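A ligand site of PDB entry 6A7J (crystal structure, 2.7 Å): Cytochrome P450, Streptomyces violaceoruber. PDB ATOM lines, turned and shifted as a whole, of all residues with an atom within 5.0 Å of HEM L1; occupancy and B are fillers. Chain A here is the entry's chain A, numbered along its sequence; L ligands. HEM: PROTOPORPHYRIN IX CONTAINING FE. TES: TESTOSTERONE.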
ATOM      1  N   LEU A  52      -7.450  18.393  -5.051  1.00  0.00           N
ATOM      2  CA  LEU A  52      -7.374  18.047  -3.678  1.00  0.00           C
ATOM      3  C   LEU A  52      -7.616  16.551  -3.451  1.00  0.00           C
ATOM      4  O   LEU A  52      -7.145  16.036  -2.472  1.00  0.00           O
ATOM      5  CB  LEU A  52      -8.327  18.918  -2.864  1.00  0.00           C
ATOM      6  CG  LEU A  52      -7.882  20.370  -2.610  1.00  0.00           C
ATOM      7  CD1 LEU A  52      -9.066  21.281  -2.295  1.00  0.00           C
ATOM      8  CD2 LEU A  52      -6.829  20.451  -1.498  1.00  0.00           C
ATOM      9  N   LYS A  59       2.195  16.290  -0.620  1.00  0.00           N
ATOM     10  CA  LYS A  59       2.756  17.252   0.316  1.00  0.00           C
ATOM     11  C   LYS A  59       4.243  17.041   0.597  1.00  0.00           C
ATOM     12  O   LYS A  59       4.799  17.720   1.443  1.00  0.00           O
ATOM     13  CB  LYS A  59       2.017  17.127   1.633  1.00  0.00           C
ATOM     14  CG  LYS A  59       0.529  17.407   1.519  1.00  0.00           C
ATOM     15  CD  LYS A  59       0.229  18.902   1.595  1.00  0.00           C
ATOM     16  CE  LYS A  59      -1.213  19.141   2.006  1.00  0.00           C
ATOM     17  NZ  LYS A  59      -1.469  20.473   2.612  1.00  0.00           N
ATOM     18  N   MET A  88       0.550  15.627  10.726  1.00  0.00           N
ATOM     19  CA  MET A  88      -0.630  15.284   9.907  1.00  0.00           C
ATOM     20  C   MET A  88      -0.663  16.054   8.572  1.00  0.00           C
ATOM     21  O   MET A  88      -0.979  15.480   7.514  1.00  0.00           O
ATOM     22  CB  MET A  88      -1.851  15.589  10.787  1.00  0.00           C
ATOM     23  CG  MET A  88      -3.236  15.647  10.140  1.00  0.00           C
ATOM     24  SD  MET A  88      -4.555  15.804  11.374  1.00  0.00           S
ATOM     25  CE  MET A  88      -3.748  16.570  12.798  1.00  0.00           C
ATOM     26  N   LEU A  89      -0.309  17.341   8.632  1.00  0.00           N
ATOM     27  CA  LEU A  89      -0.381  18.305   7.515  1.00  0.00           C
ATOM     28  C   LEU A  89       0.461  17.996   6.252  1.00  0.00           C
ATOM     29  O   LEU A  89       0.110  18.361   5.118  1.00  0.00           O
ATOM     30  CB  LEU A  89       0.027  19.695   8.067  1.00  0.00           C
ATOM     31  CG  LEU A  89       0.113  20.921   7.139  1.00  0.00           C
ATOM     32  CD1 LEU A  89      -1.244  21.286   6.530  1.00  0.00           C
ATOM     33  CD2 LEU A  89       0.719  22.078   7.907  1.00  0.00           C
ATOM     34  N   HIS A  96      -0.729   9.075   6.594  1.00  0.00           N
ATOM     35  CA  HIS A  96      -1.573  10.197   7.068  1.00  0.00           C
ATOM     36  C   HIS A  96      -2.575   9.770   8.135  1.00  0.00           C
ATOM     37  O   HIS A  96      -2.512  10.240   9.283  1.00  0.00           O
ATOM     38  CB  HIS A  96      -2.287  10.837   5.854  1.00  0.00           C
ATOM     39  CG  HIS A  96      -3.126  12.027   6.189  1.00  0.00           C
ATOM     40  ND1 HIS A  96      -4.415  12.200   5.716  1.00  0.00           N
ATOM     41  CD2 HIS A  96      -2.872  13.105   6.974  1.00  0.00           C
ATOM     42  CE1 HIS A  96      -4.908  13.324   6.196  1.00  0.00           C
ATOM     43  NE2 HIS A  96      -3.996  13.886   6.968  1.00  0.00           N
ATOM     44  N   ARG A 100      -3.532  11.629  11.861  1.00  0.00           N
ATOM     45  CA  ARG A 100      -4.877  12.247  11.946  1.00  0.00           C
ATOM     46  C   ARG A 100      -5.773  11.638  13.032  1.00  0.00           C
ATOM     47  O   ARG A 100      -6.304  12.358  13.889  1.00  0.00           O
ATOM     48  CB  ARG A 100      -5.589  12.186  10.576  1.00  0.00           C
ATOM     49  CG  ARG A 100      -6.858  13.025  10.426  1.00  0.00           C
ATOM     50  CD  ARG A 100      -7.365  12.896   8.992  1.00  0.00           C
ATOM     51  NE  ARG A 100      -8.635  13.587   8.721  1.00  0.00           N
ATOM     52  CZ  ARG A 100      -8.793  14.905   8.587  1.00  0.00           C
ATOM     53  NH1 ARG A 100      -7.792  15.757   8.734  1.00  0.00           N
ATOM     54  NH2 ARG A 100     -10.009  15.383   8.312  1.00  0.00           N
ATOM     55  N   LEU A 107     -12.414  15.856  17.837  1.00  0.00           N
ATOM     56  CA  LEU A 107     -13.109  17.074  17.364  1.00  0.00           C
ATOM     57  C   LEU A 107     -14.345  16.776  16.490  1.00  0.00           C
ATOM     58  O   LEU A 107     -14.589  17.480  15.507  1.00  0.00           O
ATOM     59  CB  LEU A 107     -12.154  17.960  16.556  1.00  0.00           C
ATOM     60  CG  LEU A 107     -10.798  18.347  17.139  1.00  0.00           C
ATOM     61  CD1 LEU A 107      -9.897  18.783  15.990  1.00  0.00           C
ATOM     62  CD2 LEU A 107     -10.916  19.443  18.196  1.00  0.00           C
ATOM     63  N   ILE A 154      -8.844  26.926  22.633  1.00  0.00           N
ATOM     64  CA  ILE A 154      -7.897  25.948  22.115  1.00  0.00           C
ATOM     65  C   ILE A 154      -6.732  25.700  23.111  1.00  0.00           C
ATOM     66  O   ILE A 154      -6.197  24.593  23.163  1.00  0.00           O
ATOM     67  CB  ILE A 154      -7.437  26.346  20.692  1.00  0.00           C
ATOM     68  CG1 ILE A 154      -6.886  25.145  19.944  1.00  0.00           C
ATOM     69  CG2 ILE A 154      -6.420  27.477  20.726  1.00  0.00           C
ATOM     70  CD1 ILE A 154      -7.954  24.192  19.453  1.00  0.00           C
ATOM     71  N   LEU A 236       0.580  22.754  15.079  1.00  0.00           N
ATOM     72  CA  LEU A 236      -0.493  22.731  14.088  1.00  0.00           C
ATOM     73  C   LEU A 236      -1.859  23.054  14.688  1.00  0.00           C
ATOM     74  O   LEU A 236      -2.543  23.936  14.193  1.00  0.00           O
ATOM     75  CB  LEU A 236      -0.514  21.359  13.438  1.00  0.00           C
ATOM     76  CG  LEU A 236      -1.728  20.896  12.643  1.00  0.00           C
ATOM     77  CD1 LEU A 236      -2.076  21.857  11.535  1.00  0.00           C
ATOM     78  CD2 LEU A 236      -1.426  19.522  12.061  1.00  0.00           C
ATOM     79  N   ILE A 237      -2.224  22.367  15.767  1.00  0.00           N
ATOM     80  CA  ILE A 237      -3.523  22.545  16.417  1.00  0.00           C
ATOM     81  C   ILE A 237      -3.645  23.922  17.079  1.00  0.00           C
ATOM     82  O   ILE A 237      -4.696  24.533  16.972  1.00  0.00           O
ATOM     83  CB  ILE A 237      -3.858  21.446  17.473  1.00  0.00           C
ATOM     84  CG1 ILE A 237      -3.875  20.026  16.861  1.00  0.00           C
ATOM     85  CG2 ILE A 237      -5.212  21.701  18.133  1.00  0.00           C
ATOM     86  CD1 ILE A 237      -5.069  19.686  16.004  1.00  0.00           C
ATOM     87  N   ALA A 240      -3.492  26.767  13.707  1.00  0.00           N
ATOM     88  CA  ALA A 240      -4.666  26.709  12.802  1.00  0.00           C
ATOM     89  C   ALA A 240      -5.949  27.078  13.524  1.00  0.00           C
ATOM     90  O   ALA A 240      -6.783  27.819  12.994  1.00  0.00           O
ATOM     91  CB  ALA A 240      -4.810  25.324  12.179  1.00  0.00           C
ATOM     92  N   GLY A 241      -6.105  26.545  14.741  1.00  0.00           N
ATOM     93  CA  GLY A 241      -7.318  26.705  15.517  1.00  0.00           C
ATOM     94  C   GLY A 241      -7.557  28.015  16.256  1.00  0.00           C
ATOM     95  O   GLY A 241      -8.626  28.172  16.868  1.00  0.00           O
ATOM     96  N   THR A 244      -7.442  31.152  12.311  1.00  0.00           N
ATOM     97  CA  THR A 244      -8.565  31.180  11.388  1.00  0.00           C
ATOM     98  C   THR A 244      -9.860  31.639  12.070  1.00  0.00           C
ATOM     99  O   THR A 244     -10.565  32.481  11.545  1.00  0.00           O
ATOM    100  CB  THR A 244      -8.778  29.832  10.672  1.00  0.00           C
ATOM    101  OG1 THR A 244      -8.843  28.775  11.636  1.00  0.00           O
ATOM    102  CG2 THR A 244      -7.660  29.557   9.698  1.00  0.00           C
ATOM    103  N   THR A 245     -10.147  31.163  13.263  1.00  0.00           N
ATOM    104  CA  THR A 245     -11.484  31.338  13.807  1.00  0.00           C
ATOM    105  C   THR A 245     -11.687  32.801  14.203  1.00  0.00           C
ATOM    106  O   THR A 245     -12.791  33.373  14.026  1.00  0.00           O
ATOM    107  CB  THR A 245     -11.758  30.405  14.992  1.00  0.00           C
ATOM    108  OG1 THR A 245     -10.931  30.798  16.067  1.00  0.00           O
ATOM    109  CG2 THR A 245     -11.413  28.981  14.649  1.00  0.00           C
ATOM    110  N   LEU A 248     -12.670  34.547  11.049  1.00  0.00           N
ATOM    111  CA  LEU A 248     -14.085  34.255  10.849  1.00  0.00           C
ATOM    112  C   LEU A 248     -15.009  35.167  11.652  1.00  0.00           C
ATOM    113  O   LEU A 248     -15.966  35.715  11.091  1.00  0.00           O
ATOM    114  CB  LEU A 248     -14.400  32.823  11.191  1.00  0.00           C
ATOM    115  CG  LEU A 248     -15.841  32.473  10.863  1.00  0.00           C
ATOM    116  CD1 LEU A 248     -16.170  32.665   9.377  1.00  0.00           C
ATOM    117  CD2 LEU A 248     -16.083  31.032  11.257  1.00  0.00           C
ATOM    118  N   LEU A 281     -17.857  32.236   5.305  1.00  0.00           N
ATOM    119  CA  LEU A 281     -16.753  31.352   4.893  1.00  0.00           C
ATOM    120  C   LEU A 281     -16.582  31.198   3.406  1.00  0.00           C
ATOM    121  O   LEU A 281     -15.485  30.985   2.924  1.00  0.00           O
ATOM    122  CB  LEU A 281     -16.909  29.953   5.453  1.00  0.00           C
ATOM    123  CG  LEU A 281     -16.683  29.944   6.951  1.00  0.00           C
ATOM    124  CD1 LEU A 281     -17.371  28.729   7.529  1.00  0.00           C
ATOM    125  CD2 LEU A 281     -15.195  29.950   7.286  1.00  0.00           C
ATOM    126  N   THR A 285     -13.532  33.989   3.082  1.00  0.00           N
ATOM    127  CA  THR A 285     -12.815  33.007   3.885  1.00  0.00           C
ATOM    128  C   THR A 285     -11.723  33.673   4.678  1.00  0.00           C
ATOM    129  O   THR A 285     -11.082  34.596   4.200  1.00  0.00           O
ATOM    130  CB  THR A 285     -12.091  31.953   3.030  1.00  0.00           C
ATOM    131  OG1 THR A 285     -12.885  31.642   1.878  1.00  0.00           O
ATOM    132  CG2 THR A 285     -11.818  30.662   3.862  1.00  0.00           C
ATOM    133  N   PRO A 286     -11.480  33.184   5.891  1.00  0.00           N
ATOM    134  CA  PRO A 286     -10.290  33.570   6.628  1.00  0.00           C
ATOM    135  C   PRO A 286      -8.930  33.215   5.954  1.00  0.00           C
ATOM    136  O   PRO A 286      -7.935  33.870   6.235  1.00  0.00           O
ATOM    137  CB  PRO A 286     -10.427  32.785   7.925  1.00  0.00           C
ATOM    138  CG  PRO A 286     -11.876  32.615   8.113  1.00  0.00           C
ATOM    139  CD  PRO A 286     -12.477  32.522   6.741  1.00  0.00           C
ATOM    140  N   THR A 287      -8.888  32.192   5.107  1.00  0.00           N
ATOM    141  CA  THR A 287      -7.632  31.695   4.557  1.00  0.00           C
ATOM    142  C   THR A 287      -7.648  31.902   3.028  1.00  0.00           C
ATOM    143  O   THR A 287      -8.236  31.114   2.283  1.00  0.00           O
ATOM    144  CB  THR A 287      -7.361  30.204   4.975  1.00  0.00           C
ATOM    145  OG1 THR A 287      -6.934  30.139   6.352  1.00  0.00           O
ATOM    146  CG2 THR A 287      -6.259  29.550   4.116  1.00  0.00           C
ATOM    147  N   VAL A 290      -3.851  28.471   0.646  1.00  0.00           N
ATOM    148  CA  VAL A 290      -3.227  27.387   1.434  1.00  0.00           C
ATOM    149  C   VAL A 290      -2.017  26.863   0.718  1.00  0.00           C
ATOM    150  O   VAL A 290      -2.116  26.408  -0.446  1.00  0.00           O
ATOM    151  CB  VAL A 290      -4.140  26.177   1.735  1.00  0.00           C
ATOM    152  CG1 VAL A 290      -3.365  25.133   2.536  1.00  0.00           C
ATOM    153  CG2 VAL A 290      -5.314  26.653   2.554  1.00  0.00           C
ATOM    154  N   ARG A 293       1.449  21.982  -2.241  1.00  0.00           N
ATOM    155  CA  ARG A 293       1.380  20.656  -2.752  1.00  0.00           C
ATOM    156  C   ARG A 293       2.287  20.603  -3.982  1.00  0.00           C
ATOM    157  O   ARG A 293       2.689  21.643  -4.499  1.00  0.00           O
ATOM    158  CB  ARG A 293      -0.039  20.364  -3.194  1.00  0.00           C
ATOM    159  CG  ARG A 293      -0.968  20.052  -2.034  1.00  0.00           C
ATOM    160  CD  ARG A 293      -2.433  20.197  -2.447  1.00  0.00           C
ATOM    161  NE  ARG A 293      -3.302  19.830  -1.325  1.00  0.00           N
ATOM    162  CZ  ARG A 293      -3.508  20.561  -0.241  1.00  0.00           C
ATOM    163  NH1 ARG A 293      -2.932  21.767  -0.066  1.00  0.00           N
ATOM    164  NH2 ARG A 293      -4.308  20.085   0.692  1.00  0.00           N
ATOM    165  N   PHE A 316      -8.341  29.637  -1.957  1.00  0.00           N
ATOM    166  CA  PHE A 316      -9.707  29.499  -1.414  1.00  0.00           C
ATOM    167  C   PHE A 316     -10.498  30.785  -1.503  1.00  0.00           C
ATOM    168  O   PHE A 316     -11.700  30.763  -1.768  1.00  0.00           O
ATOM    169  CB  PHE A 316      -9.709  28.985   0.037  1.00  0.00           C
ATOM    170  CG  PHE A 316      -9.409  27.532   0.153  1.00  0.00           C
ATOM    171  CD1 PHE A 316     -10.318  26.606  -0.317  1.00  0.00           C
ATOM    172  CD2 PHE A 316      -8.196  27.097   0.668  1.00  0.00           C
ATOM    173  CE1 PHE A 316     -10.026  25.258  -0.257  1.00  0.00           C
ATOM    174  CE2 PHE A 316      -7.913  25.756   0.756  1.00  0.00           C
ATOM    175  CZ  PHE A 316      -8.823  24.830   0.286  1.00  0.00           C
ATOM    176  N   ALA A 344     -14.199  26.131   2.089  1.00  0.00           N
ATOM    177  CA  ALA A 344     -13.323  26.914   2.981  1.00  0.00           C
ATOM    178  C   ALA A 344     -12.520  26.073   3.948  1.00  0.00           C
ATOM    179  O   ALA A 344     -11.511  26.530   4.468  1.00  0.00           O
ATOM    180  CB  ALA A 344     -14.135  27.943   3.751  1.00  0.00           C
ATOM    181  N   PHE A 345     -13.011  24.866   4.190  1.00  0.00           N
ATOM    182  CA  PHE A 345     -12.394  23.907   5.094  1.00  0.00           C
ATOM    183  C   PHE A 345     -11.538  22.838   4.431  1.00  0.00           C
ATOM    184  O   PHE A 345     -10.920  22.045   5.128  1.00  0.00           O
ATOM    185  CB  PHE A 345     -13.509  23.215   5.865  1.00  0.00           C
ATOM    186  CG  PHE A 345     -14.092  24.050   6.969  1.00  0.00           C
ATOM    187  CD1 PHE A 345     -13.273  24.505   8.005  1.00  0.00           C
ATOM    188  CD2 PHE A 345     -15.436  24.337   7.002  1.00  0.00           C
ATOM    189  CE1 PHE A 345     -13.801  25.260   9.042  1.00  0.00           C
ATOM    190  CE2 PHE A 345     -15.962  25.078   8.039  1.00  0.00           C
ATOM    191  CZ  PHE A 345     -15.143  25.540   9.063  1.00  0.00           C
ATOM    192  N   GLY A 346     -11.463  22.823   3.110  1.00  0.00           N
ATOM    193  CA  GLY A 346     -10.591  21.892   2.409  1.00  0.00           C
ATOM    194  C   GLY A 346     -11.393  20.792   1.771  1.00  0.00           C
ATOM    195  O   GLY A 346     -12.618  20.840   1.777  1.00  0.00           O
ATOM    196  N   PRO A 349      -8.381  14.141   1.710  1.00  0.00           N
ATOM    197  CA  PRO A 349      -7.765  13.658   2.938  1.00  0.00           C
ATOM    198  C   PRO A 349      -7.445  14.662   3.996  1.00  0.00           C
ATOM    199  O   PRO A 349      -7.568  14.341   5.168  1.00  0.00           O
ATOM    200  CB  PRO A 349      -6.485  13.030   2.438  1.00  0.00           C
ATOM    201  CG  PRO A 349      -6.883  12.448   1.103  1.00  0.00           C
ATOM    202  CD  PRO A 349      -7.971  13.312   0.554  1.00  0.00           C
ATOM    203  N   HIS A 350      -7.089  15.877   3.600  1.00  0.00           N
ATOM    204  CA  HIS A 350      -6.663  16.883   4.585  1.00  0.00           C
ATOM    205  C   HIS A 350      -7.759  17.813   5.079  1.00  0.00           C
ATOM    206  O   HIS A 350      -7.504  18.705   5.876  1.00  0.00           O
ATOM    207  CB  HIS A 350      -5.506  17.674   4.021  1.00  0.00           C
ATOM    208  CG  HIS A 350      -4.293  16.851   3.818  1.00  0.00           C
ATOM    209  ND1 HIS A 350      -3.256  16.808   4.734  1.00  0.00           N
ATOM    210  CD2 HIS A 350      -3.956  16.000   2.812  1.00  0.00           C
ATOM    211  CE1 HIS A 350      -2.323  15.981   4.299  1.00  0.00           C
ATOM    212  NE2 HIS A 350      -2.726  15.476   3.142  1.00  0.00           N
ATOM    213  N   VAL A 351      -8.985  17.596   4.643  1.00  0.00           N
ATOM    214  CA  VAL A 351     -10.086  18.472   5.019  1.00  0.00           C
ATOM    215  C   VAL A 351     -10.083  18.706   6.523  1.00  0.00           C
ATOM    216  O   VAL A 351      -9.722  17.836   7.285  1.00  0.00           O
ATOM    217  CB  VAL A 351     -11.427  17.919   4.530  1.00  0.00           C
ATOM    218  CG1 VAL A 351     -11.819  16.666   5.302  1.00  0.00           C
ATOM    219  CG2 VAL A 351     -12.494  18.978   4.619  1.00  0.00           C
ATOM    220  N   CYS A 352     -10.470  19.896   6.933  1.00  0.00           N
ATOM    221  CA  CYS A 352     -10.382  20.305   8.330  1.00  0.00           C
ATOM    222  C   CYS A 352     -11.022  19.289   9.273  1.00  0.00           C
ATOM    223  O   CYS A 352     -12.175  18.905   9.084  1.00  0.00           O
ATOM    224  CB  CYS A 352     -11.019  21.656   8.597  1.00  0.00           C
ATOM    225  SG  CYS A 352     -10.266  22.457  10.023  1.00  0.00           S
ATOM    226  N   PRO A 353     -10.271  18.850  10.266  1.00  0.00           N
ATOM    227  CA  PRO A 353     -10.817  18.047  11.349  1.00  0.00           C
ATOM    228  C   PRO A 353     -11.468  18.863  12.460  1.00  0.00           C
ATOM    229  O   PRO A 353     -12.224  18.303  13.250  1.00  0.00           O
ATOM    230  CB  PRO A 353      -9.580  17.345  11.895  1.00  0.00           C
ATOM    231  CG  PRO A 353      -8.474  18.302  11.632  1.00  0.00           C
ATOM    232  CD  PRO A 353      -8.815  19.016  10.365  1.00  0.00           C
ATOM    233  N   GLY A 354     -11.164  20.157  12.549  1.00  0.00           N
ATOM    234  CA  GLY A 354     -11.766  21.056  13.527  1.00  0.00           C
ATOM    235  C   GLY A 354     -12.908  21.948  13.018  1.00  0.00           C
ATOM    236  O   GLY A 354     -13.256  22.922  13.689  1.00  0.00           O
ATOM    237  N   LEU A 357     -15.594  22.500  15.577  1.00  0.00           N
ATOM    238  CA  LEU A 357     -15.194  23.291  16.744  1.00  0.00           C
ATOM    239  C   LEU A 357     -15.409  24.747  16.508  1.00  0.00           C
ATOM    240  O   LEU A 357     -15.990  25.416  17.353  1.00  0.00           O
ATOM    241  CB  LEU A 357     -13.737  23.108  17.120  1.00  0.00           C
ATOM    242  CG  LEU A 357     -13.290  23.944  18.335  1.00  0.00           C
ATOM    243  CD1 LEU A 357     -14.117  23.681  19.594  1.00  0.00           C
ATOM    244  CD2 LEU A 357     -11.845  23.694  18.716  1.00  0.00           C
ATOM    245  N   SER A 358     -14.927  25.251  15.384  1.00  0.00           N
ATOM    246  CA  SER A 358     -15.033  26.665  15.068  1.00  0.00           C
ATOM    247  C   SER A 358     -16.486  27.037  14.747  1.00  0.00           C
ATOM    248  O   SER A 358     -16.958  28.085  15.201  1.00  0.00           O
ATOM    249  CB  SER A 358     -14.101  27.049  13.931  1.00  0.00           C
ATOM    250  OG  SER A 358     -14.440  26.297  12.793  1.00  0.00           O
HETATM  251  CHA HEM L   1      -6.732  21.841   7.783  1.00  0.00           C
HETATM  252  CHB HEM L   1      -9.392  25.788   7.101  1.00  0.00           C
HETATM  253  CHC HEM L   1     -10.285  25.825  11.873  1.00  0.00           C
HETATM  254  CHD HEM L   1      -7.193  22.280  12.543  1.00  0.00           C
HETATM  255  C1A HEM L   1      -7.435  22.875   7.210  1.00  0.00           C
HETATM  256  C2A HEM L   1      -7.432  23.141   5.825  1.00  0.00           C
HETATM  257  C3A HEM L   1      -8.171  24.252   5.600  1.00  0.00           C
HETATM  258  C4A HEM L   1      -8.618  24.690   6.874  1.00  0.00           C
HETATM  259  CMA HEM L   1      -8.438  24.860   4.235  1.00  0.00           C
HETATM  260  CAA HEM L   1      -6.788  22.304   4.767  1.00  0.00           C
HETATM  261  CBA HEM L   1      -5.248  22.377   4.678  1.00  0.00           C
HETATM  262  CGA HEM L   1      -4.856  21.777   3.341  1.00  0.00           C
HETATM  263  O1A HEM L   1      -3.724  21.956   2.847  1.00  0.00           O
HETATM  264  O2A HEM L   1      -5.665  21.083   2.666  1.00  0.00           O
HETATM  265  C1B HEM L   1      -9.872  26.143   8.370  1.00  0.00           C
HETATM  266  C2B HEM L   1     -10.728  27.248   8.586  1.00  0.00           C
HETATM  267  C3B HEM L   1     -11.001  27.281   9.927  1.00  0.00           C
HETATM  268  C4B HEM L   1     -10.279  26.128  10.516  1.00  0.00           C
HETATM  269  CMB HEM L   1     -11.229  28.192   7.511  1.00  0.00           C
HETATM  270  CAB HEM L   1     -11.852  28.176  10.737  1.00  0.00           C
HETATM  271  CBB HEM L   1     -12.632  29.151  10.286  1.00  0.00           C
HETATM  272  C1C HEM L   1      -9.551  24.856  12.513  1.00  0.00           C
HETATM  273  C2C HEM L   1      -9.631  24.469  13.865  1.00  0.00           C
HETATM  274  C3C HEM L   1      -8.701  23.454  14.059  1.00  0.00           C
HETATM  275  C4C HEM L   1      -8.105  23.254  12.786  1.00  0.00           C
HETATM  276  CMC HEM L   1     -10.515  25.087  14.927  1.00  0.00           C
HETATM  277  CAC HEM L   1      -8.357  22.645  15.266  1.00  0.00           C
HETATM  278  CBC HEM L   1      -8.977  22.658  16.439  1.00  0.00           C
HETATM  279  C1D HEM L   1      -6.832  21.898  11.277  1.00  0.00           C
HETATM  280  C2D HEM L   1      -5.900  20.814  11.096  1.00  0.00           C
HETATM  281  C3D HEM L   1      -5.744  20.662   9.780  1.00  0.00           C
HETATM  282  C4D HEM L   1      -6.618  21.681   9.168  1.00  0.00           C
HETATM  283  CMD HEM L   1      -5.262  20.015  12.200  1.00  0.00           C
HETATM  284  CAD HEM L   1      -4.841  19.650   9.083  1.00  0.00           C
HETATM  285  CBD HEM L   1      -5.618  18.363   8.745  1.00  0.00           C
HETATM  286  CGD HEM L   1      -4.945  17.475   7.723  1.00  0.00           C
HETATM  287  O1D HEM L   1      -5.433  16.332   7.501  1.00  0.00           O
HETATM  288  O2D HEM L   1      -3.910  17.878   7.094  1.00  0.00           O
HETATM  289  NA  HEM L   1      -8.152  23.859   7.850  1.00  0.00           N
HETATM  290  NB  HEM L   1      -9.639  25.522   9.535  1.00  0.00           N
HETATM  291  NC  HEM L   1      -8.667  24.101  11.875  1.00  0.00           N
HETATM  292  ND  HEM L   1      -7.260  22.386  10.114  1.00  0.00           N
HETATM  293 FE   HEM L   1      -8.482  23.816   9.827  1.00  0.00          FE
HETATM  294  C1  TES L   2      -3.939  25.338   8.450  1.00  0.00           C
HETATM  295  C2  TES L   2      -5.044  25.559   7.422  1.00  0.00           C
HETATM  296  C3  TES L   2      -5.464  26.996   7.436  1.00  0.00           C
HETATM  297  O3  TES L   2      -6.558  27.295   6.974  1.00  0.00           O
HETATM  298  C4  TES L   2      -4.512  27.995   7.954  1.00  0.00           C
HETATM  299  C5  TES L   2      -3.239  27.663   8.235  1.00  0.00           C
HETATM  300  C6  TES L   2      -2.211  28.735   8.397  1.00  0.00           C
HETATM  301  C7  TES L   2      -1.433  28.482   9.676  1.00  0.00           C
HETATM  302  C8  TES L   2      -0.669  27.191   9.537  1.00  0.00           C
HETATM  303  C9  TES L   2      -1.718  26.082   9.427  1.00  0.00           C
HETATM  304  C10 TES L   2      -2.734  26.250   8.273  1.00  0.00           C
HETATM  305  C11 TES L   2      -0.973  24.755   9.373  1.00  0.00           C
HETATM  306  C12 TES L   2      -0.049  24.574  10.594  1.00  0.00           C
HETATM  307  C13 TES L   2       1.002  25.648  10.684  1.00  0.00           C
HETATM  308  C14 TES L   2       0.249  26.951  10.733  1.00  0.00           C
HETATM  309  C15 TES L   2       1.378  27.909  11.049  1.00  0.00           C
HETATM  310  C16 TES L   2       2.255  27.161  12.066  1.00  0.00           C
HETATM  311  C17 TES L   2       1.781  25.711  12.015  1.00  0.00           C
HETATM  312  O17 TES L   2       2.867  24.764  12.180  1.00  0.00           O
HETATM  313  C18 TES L   2       1.934  25.542   9.482  1.00  0.00           C
HETATM  314  C19 TES L   2      -2.082  25.935   6.912  1.00  0.00           C
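An iron atom (FE) of HEM L1 is bound by the side-chain sulfur of Cys 352, 2.3 Å away.
The guanidinium group (NH2) of Arg 293 lies within salt-bridge range of an oxygen (O2A) of HEM L1 (2.6 Å).
O2D of HEM L1 is in hydrogen-bond range of ND1 of His 350 (2.7 Å).
NZ of Lys 59 lies within salt-bridge range of O1A of HEM L1, at 2.7 Å.
An oxygen (O1D) of HEM L1 lies within salt-bridge range of the guanidinium group of Arg 100, 2.7 Å away.
NE2 of His 96 is in hydrogen-bond range of O1D of HEM L1, 2.9 Å away.
O3 of TES L2 is in hydrogen-bond range of OG1 of Thr 287 (2.9 Å).
The backbone carbonyl oxygen (O) of Phe 345 is in hydrogen-bond range of the backbone NH (N) of Cys 352, 2.8 Å away.
SG of Cys 352 sits close to N of Gly 354, at 3.5 Å.
The guanidinium group (NH2) of Arg 100 sits at hydrogen-bond distance from the backbone carbonyl oxygen (O) of Val 351 (2.7 Å).
NE2 of His 96 lies close to O of Met 88.
The side-chain hydroxyl (OG1) of Thr 244 sits at hydrogen-bond distance from the backbone carbonyl oxygen (O) of Ala 240, at 2.6 Å.
CG of Met 88 touches CGD of HEM L1, 3.5 Å away.
CA of Leu 89 touches O2D of HEM L1 (3.6 Å).
Ile 154 touches HEM L1 (CD1 to CBC, 3.5 Å).
Leu 236 touches HEM L1 (CG to CMD, 3.7 Å).
Ile 237 touches HEM L1.
Ala 240 touches HEM L1.
CA of Gly 241 touches C2C of HEM L1 (3.6 Å).
Thr 244 touches HEM L1.
Val 290 touches HEM L1 (CG1 to O1A, 3.2 Å).
Phe 316 touches HEM L1.
Ala 344 touches HEM L1.
O of Phe 345 touches C3A of HEM L1, 3.6 Å away.
Gly 346 touches HEM L1.
Pro 349 touches HEM L1.
Pro 353 touches HEM L1.
Gly 354 touches HEM L1 (O to CMC, 3.7 Å).
Leu 357 touches HEM L1.
OG of Ser 358 touches CAB of HEM L1, 3.8 Å away.
Hydrophobic or aromatic side chains that line HEM L1: Met 88, His 96, Ile 154, Leu 236, Ile 237, Ala 240, Val 290, Phe 316, Phe 345, His 350, Pro 353 and Leu 357.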
